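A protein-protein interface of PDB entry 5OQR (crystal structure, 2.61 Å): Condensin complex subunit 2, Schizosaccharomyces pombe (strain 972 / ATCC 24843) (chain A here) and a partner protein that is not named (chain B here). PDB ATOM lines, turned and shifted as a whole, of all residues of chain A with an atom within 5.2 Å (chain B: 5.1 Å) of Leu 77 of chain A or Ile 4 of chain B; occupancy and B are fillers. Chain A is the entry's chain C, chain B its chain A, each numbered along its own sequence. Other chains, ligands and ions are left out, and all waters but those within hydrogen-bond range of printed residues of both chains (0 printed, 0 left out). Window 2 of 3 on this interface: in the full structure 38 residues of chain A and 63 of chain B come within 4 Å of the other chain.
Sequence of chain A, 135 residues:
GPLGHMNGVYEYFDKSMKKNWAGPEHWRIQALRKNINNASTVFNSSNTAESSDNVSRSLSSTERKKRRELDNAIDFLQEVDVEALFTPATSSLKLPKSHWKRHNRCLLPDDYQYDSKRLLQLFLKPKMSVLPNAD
Among the printed residues, pairs that only touch across the chains: Phe 76 of chain A with Ile 4 of chain B (2.9 Å), Phe 76 of chain A with Ile 43 of chain B (3.0 Å), Phe 76 of chain A with Ser 8 of chain B (3.4 Å), Phe 76 of chain A with Ala 40 of chain B (3.6 Å), Gln 78 of chain A with Ile 43 of chain B (3.8 Å), Asp 75 of chain A with Ile 43 of chain B (3.8 Å) and Leu 77 of chain A with Ile 4 of chain B (3.9 Å).
Printed residues of chain B within 4 Å of Leu 77 of chain A: Ile 4 (3.9 Å).
Of chain A, only Phe 76 (2.9 Å) and Leu 77 (3.9 Å) come within 4 Å of Ile 4 of chain B.
Of the printed residues of chain A, Ile 43 of chain B touches Asp 75, Phe 76 and Gln 78.
Of the printed residues of chain B, Gln 78 of chain A touches Ile 43 (3.8 Å).
Of the printed residues of chain B, Asp 75 of chain A touches Ile 43 (3.8 Å).
Asp 36 of chain B touches none of the printed residues of chain A.
The nearest printed residue of chain B that does not touch Phe 76 of chain A is Arg 39 of chain B (4.4 Å).
The backbone carbonyl oxygen (O) of Asp 75 of chain A sits close to the side-chain amide oxygen (OE1) of Gln 78 of chain A (3.1 Å).
Of the 5 printed residues of chain A, 4 touch a printed residue of chain B.
Hydrophobic or aromatic side chains of chain A that line the printed part of chain B: Phe 76 and Leu 77.
Along chain A the printed residues that touch a printed residue of chain B span positions 75 to 78.
Hydrophobic or aromatic side chains of chain B that line the printed part of chain A: Ile 4 and Ile 43.
Among the printed residues, 7 pairs touch across the chains.
Among the printed residues, no Asp or Glu carboxylate lies within 4 Å of a Lys or Arg side-chain nitrogen of the other chain.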
ATOM      1  N   ASP A  75     -26.323   4.788   1.830  1.00  0.00           N
ATOM      2  CA  ASP A  75     -26.443   3.345   2.011  1.00  0.00           C
ATOM      3  C   ASP A  75     -27.733   2.906   1.332  1.00  0.00           C
ATOM      4  O   ASP A  75     -28.828   3.183   1.832  1.00  0.00           O
ATOM      5  CB  ASP A  75     -26.450   2.973   3.492  1.00  0.00           C
ATOM      6  CG  ASP A  75     -26.652   1.487   3.718  1.00  0.00           C
ATOM      7  OD1 ASP A  75     -26.059   0.682   2.970  1.00  0.00           O
ATOM      8  OD2 ASP A  75     -27.412   1.124   4.640  1.00  0.00           O
ATOM      9  N   PHE A  76     -27.605   2.225   0.196  1.00  0.00           N
ATOM     10  CA  PHE A  76     -28.767   1.849  -0.599  1.00  0.00           C
ATOM     11  C   PHE A  76     -29.449   0.576  -0.108  1.00  0.00           C
ATOM     12  O   PHE A  76     -30.381   0.103  -0.765  1.00  0.00           O
ATOM     13  CB  PHE A  76     -28.363   1.690  -2.066  1.00  0.00           C
ATOM     14  CG  PHE A  76     -28.239   2.992  -2.795  1.00  0.00           C
ATOM     15  CD1 PHE A  76     -29.325   3.527  -3.468  1.00  0.00           C
ATOM     16  CD2 PHE A  76     -27.044   3.689  -2.797  1.00  0.00           C
ATOM     17  CE1 PHE A  76     -29.218   4.729  -4.135  1.00  0.00           C
ATOM     18  CE2 PHE A  76     -26.932   4.891  -3.464  1.00  0.00           C
ATOM     19  CZ  PHE A  76     -28.020   5.412  -4.133  1.00  0.00           C
ATOM     20  N   LEU A  77     -29.017   0.018   1.018  1.00  0.00           N
ATOM     21  CA  LEU A  77     -29.644  -1.167   1.588  1.00  0.00           C
ATOM     22  C   LEU A  77     -30.530  -0.848   2.784  1.00  0.00           C
ATOM     23  O   LEU A  77     -31.050  -1.771   3.418  1.00  0.00           O
ATOM     24  CB  LEU A  77     -28.571  -2.184   1.991  1.00  0.00           C
ATOM     25  CG  LEU A  77     -28.112  -3.137   0.883  1.00  0.00           C
ATOM     26  CD1 LEU A  77     -27.881  -2.411  -0.442  1.00  0.00           C
ATOM     27  CD2 LEU A  77     -26.855  -3.875   1.313  1.00  0.00           C
ATOM     28  N   GLN A  78     -30.720   0.429   3.098  1.00  0.00           N
ATOM     29  CA  GLN A  78     -31.592   0.818   4.193  1.00  0.00           C
ATOM     30  C   GLN A  78     -33.039   0.454   3.877  1.00  0.00           C
ATOM     31  O   GLN A  78     -33.426   0.268   2.719  1.00  0.00           O
ATOM     32  CB  GLN A  78     -31.480   2.320   4.455  1.00  0.00           C
ATOM     33  CG  GLN A  78     -30.060   2.807   4.711  1.00  0.00           C
ATOM     34  CD  GLN A  78     -29.924   4.309   4.558  1.00  0.00           C
ATOM     35  OE1 GLN A  78     -30.555   4.916   3.693  1.00  0.00           O
ATOM     36  NE2 GLN A  78     -29.097   4.918   5.398  1.00  0.00           N
ATOM     37  N   GLU A  79     -33.845   0.354   4.929  1.00  0.00           N
ATOM     38  CA  GLU A  79     -35.260   0.043   4.789  1.00  0.00           C
ATOM     39  C   GLU A  79     -36.065   1.327   4.640  1.00  0.00           C
ATOM     40  O   GLU A  79     -35.827   2.311   5.347  1.00  0.00           O
ATOM     41  CB  GLU A  79     -35.755  -0.755   5.995  1.00  0.00           C
ATOM     42  CG  GLU A  79     -35.110  -2.127   6.125  1.00  0.00           C
ATOM     43  CD  GLU A  79     -35.543  -2.861   7.377  1.00  0.00           C
ATOM     44  OE1 GLU A  79     -36.180  -2.233   8.249  1.00  0.00           O
ATOM     45  OE2 GLU A  79     -35.248  -4.070   7.490  1.00  0.00           O
ATOM     46  N   SER B   2     -26.090  -6.569  -5.043  1.00  0.00           N
ATOM     47  CA  SER B   2     -26.147  -7.092  -6.401  1.00  0.00           C
ATOM     48  C   SER B   2     -26.559  -5.995  -7.380  1.00  0.00           C
ATOM     49  O   SER B   2     -25.888  -4.968  -7.479  1.00  0.00           O
ATOM     50  CB  SER B   2     -27.118  -8.265  -6.467  1.00  0.00           C
ATOM     51  OG  SER B   2     -28.457  -7.826  -6.312  1.00  0.00           O
ATOM     52  N   CYS B   3     -27.660  -6.218  -8.102  1.00  0.00           N
ATOM     53  CA  CYS B   3     -28.179  -5.188  -8.997  1.00  0.00           C
ATOM     54  C   CYS B   3     -28.298  -3.848  -8.283  1.00  0.00           C
ATOM     55  O   CYS B   3     -28.057  -2.792  -8.878  1.00  0.00           O
ATOM     56  CB  CYS B   3     -29.534  -5.621  -9.553  1.00  0.00           C
ATOM     57  SG  CYS B   3     -30.453  -4.303 -10.374  1.00  0.00           S
ATOM     58  N   ILE B   4     -28.665  -3.870  -7.001  1.00  0.00           N
ATOM     59  CA  ILE B   4     -28.735  -2.631  -6.239  1.00  0.00           C
ATOM     60  C   ILE B   4     -27.340  -2.151  -5.859  1.00  0.00           C
ATOM     61  O   ILE B   4     -27.103  -0.941  -5.769  1.00  0.00           O
ATOM     62  CB  ILE B   4     -29.622  -2.807  -4.994  1.00  0.00           C
ATOM     63  CG1 ILE B   4     -29.987  -1.435  -4.419  1.00  0.00           C
ATOM     64  CG2 ILE B   4     -28.924  -3.682  -3.948  1.00  0.00           C
ATOM     65  CD1 ILE B   4     -30.883  -1.481  -3.199  1.00  0.00           C
ATOM     66  N   GLN B   5     -26.401  -3.071  -5.627  1.00  0.00           N
ATOM     67  CA  GLN B   5     -25.055  -2.666  -5.239  1.00  0.00           C
ATOM     68  C   GLN B   5     -24.261  -2.123  -6.419  1.00  0.00           C
ATOM     69  O   GLN B   5     -23.370  -1.289  -6.224  1.00  0.00           O
ATOM     70  CB  GLN B   5     -24.306  -3.836  -4.600  1.00  0.00           C
ATOM     71  CG  GLN B   5     -24.699  -4.094  -3.151  1.00  0.00           C
ATOM     72  CD  GLN B   5     -23.611  -4.803  -2.368  1.00  0.00           C
ATOM     73  OE1 GLN B   5     -22.547  -5.115  -2.900  1.00  0.00           O
ATOM     74  NE2 GLN B   5     -23.872  -5.055  -1.090  1.00  0.00           N
ATOM     75  N   ILE B   6     -24.551  -2.585  -7.637  1.00  0.00           N
ATOM     76  CA  ILE B   6     -23.984  -1.942  -8.820  1.00  0.00           C
ATOM     77  C   ILE B   6     -24.312  -0.457  -8.793  1.00  0.00           C
ATOM     78  O   ILE B   6     -23.448   0.400  -9.009  1.00  0.00           O
ATOM     79  CB  ILE B   6     -24.511  -2.601 -10.108  1.00  0.00           C
ATOM     80  CG1 ILE B   6     -24.167  -4.094 -10.139  1.00  0.00           C
ATOM     81  CG2 ILE B   6     -23.925  -1.904 -11.337  1.00  0.00           C
ATOM     82  CD1 ILE B   6     -24.864  -4.851 -11.251  1.00  0.00           C
ATOM     83  N   ILE B   7     -25.576  -0.136  -8.511  1.00  0.00           N
ATOM     84  CA  ILE B   7     -26.002   1.258  -8.436  1.00  0.00           C
ATOM     85  C   ILE B   7     -25.278   1.970  -7.301  1.00  0.00           C
ATOM     86  O   ILE B   7     -24.732   3.065  -7.477  1.00  0.00           O
ATOM     87  CB  ILE B   7     -27.531   1.333  -8.275  1.00  0.00           C
ATOM     88  CG1 ILE B   7     -28.210   0.715  -9.502  1.00  0.00           C
ATOM     89  CG2 ILE B   7     -27.979   2.776  -8.074  1.00  0.00           C
ATOM     90  CD1 ILE B   7     -29.721   0.682  -9.440  1.00  0.00           C
ATOM     91  N   SER B   8     -25.261   1.355  -6.115  1.00  0.00           N
ATOM     92  CA  SER B   8     -24.557   1.946  -4.985  1.00  0.00           C
ATOM     93  C   SER B   8     -23.083   2.182  -5.292  1.00  0.00           C
ATOM     94  O   SER B   8     -22.445   3.000  -4.621  1.00  0.00           O
ATOM     95  CB  SER B   8     -24.694   1.048  -3.753  1.00  0.00           C
ATOM     96  OG  SER B   8     -24.271   1.723  -2.582  1.00  0.00           O
ATOM     97  N   ASP B  36     -35.607  -3.791  -8.317  1.00  0.00           N
ATOM     98  CA  ASP B  36     -34.417  -3.309  -7.621  1.00  0.00           C
ATOM     99  C   ASP B  36     -34.092  -1.867  -7.983  1.00  0.00           C
ATOM    100  O   ASP B  36     -33.543  -1.131  -7.155  1.00  0.00           O
ATOM    101  CB  ASP B  36     -33.222  -4.210  -7.935  1.00  0.00           C
ATOM    102  CG  ASP B  36     -32.944  -5.218  -6.833  1.00  0.00           C
ATOM    103  OD1 ASP B  36     -33.873  -5.531  -6.059  1.00  0.00           O
ATOM    104  OD2 ASP B  36     -31.794  -5.697  -6.741  1.00  0.00           O
ATOM    105  N   ARG B  39     -36.343   0.360  -6.110  1.00  0.00           N
ATOM    106  CA  ARG B  39     -35.813   0.347  -4.752  1.00  0.00           C
ATOM    107  C   ARG B  39     -34.641   1.311  -4.616  1.00  0.00           C
ATOM    108  O   ARG B  39     -34.484   1.971  -3.583  1.00  0.00           O
ATOM    109  CB  ARG B  39     -35.392  -1.074  -4.377  1.00  0.00           C
ATOM    110  CG  ARG B  39     -34.958  -1.246  -2.938  1.00  0.00           C
ATOM    111  CD  ARG B  39     -34.478  -2.667  -2.688  1.00  0.00           C
ATOM    112  NE  ARG B  39     -33.590  -2.754  -1.532  1.00  0.00           N
ATOM    113  CZ  ARG B  39     -32.917  -3.847  -1.187  1.00  0.00           C
ATOM    114  NH1 ARG B  39     -33.023  -4.956  -1.907  1.00  0.00           N
ATOM    115  NH2 ARG B  39     -32.132  -3.832  -0.118  1.00  0.00           N
ATOM    116  N   ALA B  40     -33.804   1.402  -5.653  1.00  0.00           N
ATOM    117  CA  ALA B  40     -32.711   2.368  -5.636  1.00  0.00           C
ATOM    118  C   ALA B  40     -33.242   3.793  -5.669  1.00  0.00           C
ATOM    119  O   ALA B  40     -32.680   4.687  -5.028  1.00  0.00           O
ATOM    120  CB  ALA B  40     -31.774   2.122  -6.819  1.00  0.00           C
ATOM    121  N   ILE B  43     -34.701   5.167  -2.487  1.00  0.00           N
ATOM    122  CA  ILE B  43     -33.628   5.674  -1.636  1.00  0.00           C
ATOM    123  C   ILE B  43     -33.040   6.971  -2.173  1.00  0.00           C
ATOM    124  O   ILE B  43     -32.267   7.634  -1.463  1.00  0.00           O
ATOM    125  CB  ILE B  43     -32.561   4.571  -1.462  1.00  0.00           C
ATOM    126  CG1 ILE B  43     -33.073   3.545  -0.441  1.00  0.00           C
ATOM    127  CG2 ILE B  43     -31.197   5.152  -1.054  1.00  0.00           C
ATOM    128  CD1 ILE B  43     -32.092   2.468  -0.061  1.00  0.00           C
